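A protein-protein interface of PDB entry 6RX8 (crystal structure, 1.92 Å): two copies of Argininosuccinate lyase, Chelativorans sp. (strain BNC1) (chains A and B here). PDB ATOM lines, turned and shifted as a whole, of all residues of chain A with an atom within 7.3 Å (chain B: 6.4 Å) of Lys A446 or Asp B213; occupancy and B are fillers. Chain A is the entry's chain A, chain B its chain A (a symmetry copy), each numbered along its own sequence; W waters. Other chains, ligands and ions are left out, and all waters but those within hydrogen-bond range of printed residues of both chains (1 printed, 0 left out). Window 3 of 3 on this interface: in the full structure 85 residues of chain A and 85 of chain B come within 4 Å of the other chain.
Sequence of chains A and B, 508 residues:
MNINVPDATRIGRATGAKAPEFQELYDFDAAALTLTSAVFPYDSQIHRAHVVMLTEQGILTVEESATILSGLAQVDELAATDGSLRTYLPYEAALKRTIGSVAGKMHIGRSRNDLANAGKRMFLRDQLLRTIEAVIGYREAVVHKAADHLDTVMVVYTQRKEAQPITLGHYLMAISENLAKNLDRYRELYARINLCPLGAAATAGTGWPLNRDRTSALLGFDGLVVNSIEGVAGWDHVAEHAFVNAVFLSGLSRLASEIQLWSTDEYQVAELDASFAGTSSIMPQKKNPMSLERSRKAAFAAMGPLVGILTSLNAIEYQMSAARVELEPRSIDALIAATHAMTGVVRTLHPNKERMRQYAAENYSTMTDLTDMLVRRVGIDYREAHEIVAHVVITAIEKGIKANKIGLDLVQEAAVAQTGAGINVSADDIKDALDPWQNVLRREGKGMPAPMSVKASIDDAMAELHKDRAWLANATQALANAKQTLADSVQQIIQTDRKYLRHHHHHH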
ATOM      1  N   HIS A 170      18.923   4.771 -15.001  1.00  0.00           N
ATOM      2  CA  HIS A 170      20.232   4.147 -14.837  1.00  0.00           C
ATOM      3  C   HIS A 170      21.152   5.034 -14.006  1.00  0.00           C
ATOM      4  O   HIS A 170      21.809   4.566 -13.070  1.00  0.00           O
ATOM      5  CB  HIS A 170      20.837   3.854 -16.208  1.00  0.00           C
ATOM      6  CG  HIS A 170      22.207   3.254 -16.148  1.00  0.00           C
ATOM      7  ND1 HIS A 170      23.330   3.913 -16.597  1.00  0.00           N
ATOM      8  CD2 HIS A 170      22.635   2.058 -15.678  1.00  0.00           C
ATOM      9  CE1 HIS A 170      24.392   3.147 -16.411  1.00  0.00           C
ATOM     10  NE2 HIS A 170      23.997   2.012 -15.863  1.00  0.00           N
ATOM     11  N   ARG A 443      22.737  -2.704 -23.964  1.00  0.00           N
ATOM     12  CA  ARG A 443      23.477  -2.715 -22.705  1.00  0.00           C
ATOM     13  C   ARG A 443      22.586  -3.294 -21.610  1.00  0.00           C
ATOM     14  O   ARG A 443      22.082  -2.589 -20.729  1.00  0.00           O
ATOM     15  CB  ARG A 443      23.954  -1.311 -22.368  1.00  0.00           C
ATOM     16  CG  ARG A 443      25.060  -0.833 -23.286  1.00  0.00           C
ATOM     17  CD  ARG A 443      25.320   0.670 -23.159  1.00  0.00           C
ATOM     18  NE  ARG A 443      26.555   0.975 -23.870  1.00  0.00           N
ATOM     19  CZ  ARG A 443      26.672   0.954 -25.195  1.00  0.00           C
ATOM     20  NH1 ARG A 443      27.838   1.206 -25.768  1.00  0.00           N
ATOM     21  NH2 ARG A 443      25.617   0.689 -25.947  1.00  0.00           N
ATOM     22  N   GLU A 444      22.415  -4.615 -21.678  1.00  0.00           N
ATOM     23  CA  GLU A 444      21.424  -5.324 -20.880  1.00  0.00           C
ATOM     24  C   GLU A 444      22.028  -6.201 -19.785  1.00  0.00           C
ATOM     25  O   GLU A 444      21.289  -6.934 -19.122  1.00  0.00           O
ATOM     26  CB  GLU A 444      20.535  -6.173 -21.798  1.00  0.00           C
ATOM     27  CG  GLU A 444      21.297  -7.155 -22.697  1.00  0.00           C
ATOM     28  CD  GLU A 444      20.380  -8.149 -23.406  1.00  0.00           C
ATOM     29  OE1 GLU A 444      20.870  -9.199 -23.882  1.00  0.00           O
ATOM     30  OE2 GLU A 444      19.162  -7.880 -23.480  1.00  0.00           O
ATOM     31  N   GLY A 445      23.336  -6.136 -19.556  1.00  0.00           N
ATOM     32  CA  GLY A 445      23.940  -6.883 -18.472  1.00  0.00           C
ATOM     33  C   GLY A 445      23.685  -6.252 -17.110  1.00  0.00           C
ATOM     34  O   GLY A 445      23.002  -5.239 -16.971  1.00  0.00           O
ATOM     35  N   LYS A 446      24.263  -6.877 -16.079  1.00  0.00           N
ATOM     36  CA  LYS A 446      24.121  -6.394 -14.708  1.00  0.00           C
ATOM     37  C   LYS A 446      24.653  -4.973 -14.574  1.00  0.00           C
ATOM     38  O   LYS A 446      25.820  -4.709 -14.896  1.00  0.00           O
ATOM     39  CB  LYS A 446      24.865  -7.316 -13.744  1.00  0.00           C
ATOM     40  CG  LYS A 446      24.282  -8.711 -13.572  1.00  0.00           C
ATOM     41  CD  LYS A 446      25.183  -9.535 -12.656  1.00  0.00           C
ATOM     42  CE  LYS A 446      24.554 -10.860 -12.262  1.00  0.00           C
ATOM     43  NZ  LYS A 446      25.269 -11.455 -11.098  1.00  0.00           N
ATOM     44  N   GLY A 447      23.805  -4.070 -14.083  1.00  0.00           N
ATOM     45  CA  GLY A 447      24.197  -2.706 -13.808  1.00  0.00           C
ATOM     46  C   GLY A 447      24.208  -1.796 -15.010  1.00  0.00           C
ATOM     47  O   GLY A 447      24.709  -0.673 -14.917  1.00  0.00           O
ATOM     48  N   MET A 448      23.675  -2.234 -16.109  1.00  0.00           N
ATOM     49  CA  MET A 448      23.690  -1.492 -17.355  1.00  0.00           C
ATOM     50  C   MET A 448      22.331  -0.859 -17.602  1.00  0.00           C
ATOM     51  O   MET A 448      21.337  -1.238 -16.977  1.00  0.00           O
ATOM     52  CB  MET A 448      24.074  -2.427 -18.500  1.00  0.00           C
ATOM     53  CG  MET A 448      25.390  -3.159 -18.250  1.00  0.00           C
ATOM     54  SD  MET A 448      25.912  -4.130 -19.677  1.00  0.00           S
ATOM     55  CE  MET A 448      27.306  -5.023 -18.982  1.00  0.00           C
ATOM     56  N   PRO A 449      22.250   0.117 -18.514  1.00  0.00           N
ATOM     57  CA  PRO A 449      21.060   0.981 -18.578  1.00  0.00           C
ATOM     58  C   PRO A 449      19.816   0.382 -19.227  1.00  0.00           C
ATOM     59  O   PRO A 449      18.776   1.053 -19.230  1.00  0.00           O
ATOM     60  CB  PRO A 449      21.563   2.187 -19.398  1.00  0.00           C
ATOM     61  CG  PRO A 449      22.683   1.617 -20.260  1.00  0.00           C
ATOM     62  CD  PRO A 449      23.368   0.644 -19.323  1.00  0.00           C
ATOM     63  N   SER A 453      17.406  -4.269 -17.001  1.00  0.00           N
ATOM     64  CA  SER A 453      18.498  -4.322 -16.037  1.00  0.00           C
ATOM     65  C   SER A 453      18.328  -3.276 -14.944  1.00  0.00           C
ATOM     66  O   SER A 453      18.595  -3.546 -13.770  1.00  0.00           O
ATOM     67  CB  SER A 453      19.845  -4.104 -16.723  1.00  0.00           C
ATOM     68  OG  SER A 453      19.992  -4.933 -17.853  1.00  0.00           O
ATOM     69  N   SER A 457      17.722  -3.754 -10.760  1.00  0.00           N
ATOM     70  CA  SER A 457      18.385  -3.008  -9.698  1.00  0.00           C
ATOM     71  C   SER A 457      17.379  -2.286  -8.812  1.00  0.00           C
ATOM     72  O   SER A 457      17.585  -2.171  -7.600  1.00  0.00           O
ATOM     73  CB  SER A 457      19.362  -2.000 -10.294  1.00  0.00           C
ATOM     74  OG  SER A 457      20.455  -2.674 -10.876  1.00  0.00           O
ATOM     75  N   GLY B 199      33.269  -4.906 -16.513  1.00  0.00           N
ATOM     76  CA  GLY B 199      32.000  -4.996 -17.188  1.00  0.00           C
ATOM     77  C   GLY B 199      31.270  -3.676 -17.287  1.00  0.00           C
ATOM     78  O   GLY B 199      30.381  -3.535 -18.133  1.00  0.00           O
ATOM     79  N   ALA B 200      31.615  -2.710 -16.437  1.00  0.00           N
ATOM     80  CA  ALA B 200      31.103  -1.358 -16.601  1.00  0.00           C
ATOM     81  C   ALA B 200      31.655  -0.689 -17.851  1.00  0.00           C
ATOM     82  O   ALA B 200      31.066   0.277 -18.340  1.00  0.00           O
ATOM     83  CB  ALA B 200      31.442  -0.522 -15.369  1.00  0.00           C
ATOM     84  N   LEU B 210      29.215 -10.063 -21.917  1.00  0.00           N
ATOM     85  CA  LEU B 210      30.183 -10.400 -20.889  1.00  0.00           C
ATOM     86  C   LEU B 210      29.514 -11.191 -19.777  1.00  0.00           C
ATOM     87  O   LEU B 210      28.314 -11.056 -19.520  1.00  0.00           O
ATOM     88  CB  LEU B 210      30.815  -9.143 -20.301  1.00  0.00           C
ATOM     89  CG  LEU B 210      31.348  -8.132 -21.313  1.00  0.00           C
ATOM     90  CD1 LEU B 210      32.153  -7.063 -20.575  1.00  0.00           C
ATOM     91  CD2 LEU B 210      32.180  -8.814 -22.392  1.00  0.00           C
ATOM     92  N   ASN B 211      30.299 -12.033 -19.127  1.00  0.00           N
ATOM     93  CA  ASN B 211      29.903 -12.646 -17.867  1.00  0.00           C
ATOM     94  C   ASN B 211      30.709 -11.932 -16.787  1.00  0.00           C
ATOM     95  O   ASN B 211      31.876 -12.272 -16.543  1.00  0.00           O
ATOM     96  CB  ASN B 211      30.133 -14.151 -17.862  1.00  0.00           C
ATOM     97  CG  ASN B 211      29.649 -14.787 -16.582  1.00  0.00           C
ATOM     98  OD1 ASN B 211      29.399 -14.101 -15.587  1.00  0.00           O
ATOM     99  ND2 ASN B 211      29.525 -16.104 -16.590  1.00  0.00           N
ATOM    100  N   ARG B 212      30.100 -10.913 -16.178  1.00  0.00           N
ATOM    101  CA  ARG B 212      30.814 -10.112 -15.194  1.00  0.00           C
ATOM    102  C   ARG B 212      31.148 -10.928 -13.955  1.00  0.00           C
ATOM    103  O   ARG B 212      32.141 -10.646 -13.274  1.00  0.00           O
ATOM    104  CB  ARG B 212      29.988  -8.885 -14.809  1.00  0.00           C
ATOM    105  CG  ARG B 212      29.588  -7.986 -15.980  1.00  0.00           C
ATOM    106  CD  ARG B 212      28.976  -6.672 -15.474  1.00  0.00           C
ATOM    107  NE  ARG B 212      29.863  -6.039 -14.500  1.00  0.00           N
ATOM    108  CZ  ARG B 212      29.477  -5.216 -13.526  1.00  0.00           C
ATOM    109  NH1 ARG B 212      28.196  -4.894 -13.360  1.00  0.00           N
ATOM    110  NH2 ARG B 212      30.393  -4.725 -12.700  1.00  0.00           N
ATOM    111  N   ASP B 213      30.334 -11.938 -13.642  1.00  0.00           N
ATOM    112  CA  ASP B 213      30.608 -12.762 -12.474  1.00  0.00           C
ATOM    113  C   ASP B 213      31.877 -13.579 -12.668  1.00  0.00           C
ATOM    114  O   ASP B 213      32.642 -13.775 -11.720  1.00  0.00           O
ATOM    115  CB  ASP B 213      29.420 -13.676 -12.179  1.00  0.00           C
ATOM    116  CG  ASP B 213      28.224 -12.919 -11.637  1.00  0.00           C
ATOM    117  OD1 ASP B 213      28.423 -11.942 -10.882  1.00  0.00           O
ATOM    118  OD2 ASP B 213      27.081 -13.296 -11.964  1.00  0.00           O
ATOM    119  N   ARG B 214      32.126 -14.056 -13.891  1.00  0.00           N
ATOM    120  CA  ARG B 214      33.292 -14.901 -14.136  1.00  0.00           C
ATOM    121  C   ARG B 214      34.583 -14.097 -14.008  1.00  0.00           C
ATOM    122  O   ARG B 214      35.527 -14.533 -13.343  1.00  0.00           O
ATOM    123  CB  ARG B 214      33.187 -15.563 -15.513  1.00  0.00           C
ATOM    124  CG  ARG B 214      34.191 -16.707 -15.767  1.00  0.00           C
ATOM    125  CD  ARG B 214      33.620 -18.098 -15.393  1.00  0.00           C
ATOM    126  NE  ARG B 214      33.841 -18.381 -13.982  1.00  0.00           N
ATOM    127  CZ  ARG B 214      34.989 -18.841 -13.504  1.00  0.00           C
ATOM    128  NH1 ARG B 214      35.996 -19.092 -14.337  1.00  0.00           N
ATOM    129  NH2 ARG B 214      35.131 -19.057 -12.204  1.00  0.00           N
ATOM    130  N   THR B 215      34.644 -12.919 -14.636  1.00  0.00           N
ATOM    131  CA  THR B 215      35.817 -12.064 -14.484  1.00  0.00           C
ATOM    132  C   THR B 215      36.053 -11.730 -13.016  1.00  0.00           C
ATOM    133  O   THR B 215      37.187 -11.778 -12.524  1.00  0.00           O
ATOM    134  CB  THR B 215      35.631 -10.779 -15.286  1.00  0.00           C
ATOM    135  OG1 THR B 215      34.903 -11.067 -16.482  1.00  0.00           O
ATOM    136  CG2 THR B 215      36.969 -10.172 -15.649  1.00  0.00           C
ATOM    137  N   SER B 216      34.986 -11.380 -12.305  1.00  0.00           N
ATOM    138  CA  SER B 216      35.100 -11.100 -10.881  1.00  0.00           C
ATOM    139  C   SER B 216      35.672 -12.298 -10.132  1.00  0.00           C
ATOM    140  O   SER B 216      36.608 -12.158  -9.342  1.00  0.00           O
ATOM    141  CB  SER B 216      33.730 -10.708 -10.334  1.00  0.00           C
ATOM    142  OG  SER B 216      33.769 -10.539  -8.933  1.00  0.00           O
ATOM    143  N   ALA B 217      35.123 -13.491 -10.372  1.00  0.00           N
ATOM    144  CA  ALA B 217      35.589 -14.671  -9.650  1.00  0.00           C
ATOM    145  C   ALA B 217      37.036 -14.997  -9.997  1.00  0.00           C
ATOM    146  O   ALA B 217      37.831 -15.351  -9.118  1.00  0.00           O
ATOM    147  CB  ALA B 217      34.684 -15.863  -9.965  1.00  0.00           C
ATOM    148  N   LEU B 218      37.395 -14.886 -11.276  1.00  0.00           N
ATOM    149  CA  LEU B 218      38.762 -15.174 -11.691  1.00  0.00           C
ATOM    150  C   LEU B 218      39.757 -14.254 -11.006  1.00  0.00           C
ATOM    151  O   LEU B 218      40.919 -14.627 -10.809  1.00  0.00           O
ATOM    152  CB  LEU B 218      38.877 -15.047 -13.208  1.00  0.00           C
ATOM    153  CG  LEU B 218      38.231 -16.185 -14.003  1.00  0.00           C
ATOM    154  CD1 LEU B 218      38.101 -15.822 -15.465  1.00  0.00           C
ATOM    155  CD2 LEU B 218      39.052 -17.451 -13.817  1.00  0.00           C
ATOM    156  N   GLY B 223      32.239 -10.041  -5.011  1.00  0.00           N
ATOM    157  CA  GLY B 223      30.994  -9.476  -5.515  1.00  0.00           C
ATOM    158  C   GLY B 223      31.293  -8.460  -6.584  1.00  0.00           C
ATOM    159  O   GLY B 223      32.427  -8.270  -6.904  1.00  0.00           O
ATOM    160  N   LEU B 224      30.245  -7.883  -7.122  1.00  0.00           N
ATOM    161  CA  LEU B 224      30.321  -6.898  -8.197  1.00  0.00           C
ATOM    162  C   LEU B 224      30.001  -5.514  -7.640  1.00  0.00           C
ATOM    163  O   LEU B 224      29.273  -5.415  -6.709  1.00  0.00           O
ATOM    164  CB  LEU B 224      29.270  -7.192  -9.264  1.00  0.00           C
ATOM    165  CG  LEU B 224      29.388  -8.482 -10.063  1.00  0.00           C
ATOM    166  CD1 LEU B 224      28.483  -8.421 -11.257  1.00  0.00           C
ATOM    167  CD2 LEU B 224      30.813  -8.764 -10.482  1.00  0.00           C
ATOM    168  N   VAL B 225      30.591  -4.512  -8.226  1.00  0.00           N
ATOM    169  CA  VAL B 225      30.082  -3.146  -8.135  1.00  0.00           C
ATOM    170  C   VAL B 225      29.040  -3.266  -9.248  1.00  0.00           C
ATOM    171  O   VAL B 225      29.426  -3.450 -10.378  1.00  0.00           O
ATOM    172  CB  VAL B 225      31.108  -2.072  -8.469  1.00  0.00           C
ATOM    173  CG1 VAL B 225      30.365  -0.786  -8.462  1.00  0.00           C
ATOM    174  CG2 VAL B 225      32.322  -2.040  -7.556  1.00  0.00           C
ATOM    175  N   VAL B 226      27.776  -3.223  -8.936  1.00  0.00           N
ATOM    176  CA  VAL B 226      26.733  -3.581  -9.912  1.00  0.00           C
ATOM    177  C   VAL B 226      26.571  -2.484 -10.957  1.00  0.00           C
ATOM    178  O   VAL B 226      26.979  -2.712 -12.019  1.00  0.00           O
ATOM    179  CB  VAL B 226      25.446  -3.964  -9.171  1.00  0.00           C
ATOM    180  CG1 VAL B 226      24.343  -4.295 -10.143  1.00  0.00           C
ATOM    181  CG2 VAL B 226      25.704  -5.119  -8.217  1.00  0.00           C
ATOM    182  N   ASN B 227      26.033  -1.334 -10.584  1.00  0.00           N
ATOM    183  CA  ASN B 227      25.756  -0.209 -11.512  1.00  0.00           C
ATOM    184  C   ASN B 227      27.034   0.219 -12.248  1.00  0.00           C
ATOM    185  O   ASN B 227      27.988   0.496 -11.607  1.00  0.00           O
ATOM    186  CB  ASN B 227      25.093   0.945 -10.795  1.00  0.00           C
ATOM    187  CG  ASN B 227      24.810   2.082 -11.728  1.00  0.00           C
ATOM    188  OD1 ASN B 227      25.691   2.835 -12.036  1.00  0.00           O
ATOM    189  ND2 ASN B 227      23.581   2.173 -12.176  1.00  0.00           N
ATOM    190  N   SER B 228      26.977   0.366 -13.555  1.00  0.00           N
ATOM    191  CA  SER B 228      28.177   0.597 -14.350  1.00  0.00           C
ATOM    192  C   SER B 228      28.762   1.984 -14.120  1.00  0.00           C
ATOM    193  O   SER B 228      29.989   2.151 -14.184  1.00  0.00           O
ATOM    194  CB  SER B 228      27.857   0.396 -15.832  1.00  0.00           C
ATOM    195  OG  SER B 228      26.853   1.297 -16.263  1.00  0.00           O
HETATM  196  O   HOH W   1      21.721  -0.211 -11.993  1.00  0.00           O
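No position is printed for both chains.
The backbone carbonyl oxygen of Gly A447 is in hydrogen-bond range of a ring nitrogen (NE2) of His A170.
The backbone NH (N) of Gly A445 sits at hydrogen-bond distance from the side-chain sulfur (SD) of Met A448 (3.3 Å).
The side-chain amide oxygen (OD1) of Asn B211 is in hydrogen-bond range of the backbone NH (N) of Asp B213, 3.1 Å away.
NH2 of Arg B212 sits at hydrogen-bond distance from O of Val B225.
O of Val B226 lies within hydrogen-bond range of NH1 of Arg B212 (2.8 Å).
O of His A170 sits at hydrogen-bond distance from ND2 of Asn B227 (3.1 Å).
The side-chain hydroxyl (OG) of Ser B228 sits at hydrogen-bond distance from a ring nitrogen (NE2) of His A170 (3.0 Å).
The backbone carbonyl oxygen (O) of Lys A446 sits at hydrogen-bond distance from the guanidinium group (NH1) of Arg B212 (2.8 Å).
NZ of Lys A446 lies within salt-bridge range of OD2 of Asp B213.
O of Gly A447 is in hydrogen-bond range of N of Ser B228, 2.8 Å away.
Of chain B, only Arg B212, Asp B213, Leu B224 and Val B226 come within 4 Å of Lys A446.
Printed residues of chain B within 4 Å of Gly A447: Val B226 (3.3 Å), Asn B227 (3.6 Å) and Ser B228 (2.8 Å).
Of the printed residues of chain A, Gly B199 touches Met A448.
Ala B217 touches none of the printed residues of chain A.
The nearest residue of chain B that does not touch Lys A446 is Ser B228 (5.4 Å).
Printed residues of chain B that touch a printed residue of chain A: Gly B199, Arg B212, Asp B213, Leu B224, Val B226, Asn B227 and Ser B228.
Hydrophobic or aromatic side chains of chain B within 4 Å of the printed part of chain A: Leu B224 and Val B226.
Along chain B the printed residues that touch a printed residue of chain A span positions 199 to 228.
Hydrophobic or aromatic side chains of chain A within 4 Å of the printed part of chain B: His A170 and Met A448.
Among the printed residues, 10 pairs touch across the chains.
Among the printed residues, merely in contact across the chains: Gly A447 with Val B226, Met A448 with Gly B199, Gly A447 with Asn B227, Lys A446 with Val B226 and Lys A446 with Leu B224.
Water W1 bridges the side-chain hydroxyl of Ser A457 and the side-chain amide nitrogen of Asn B227.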
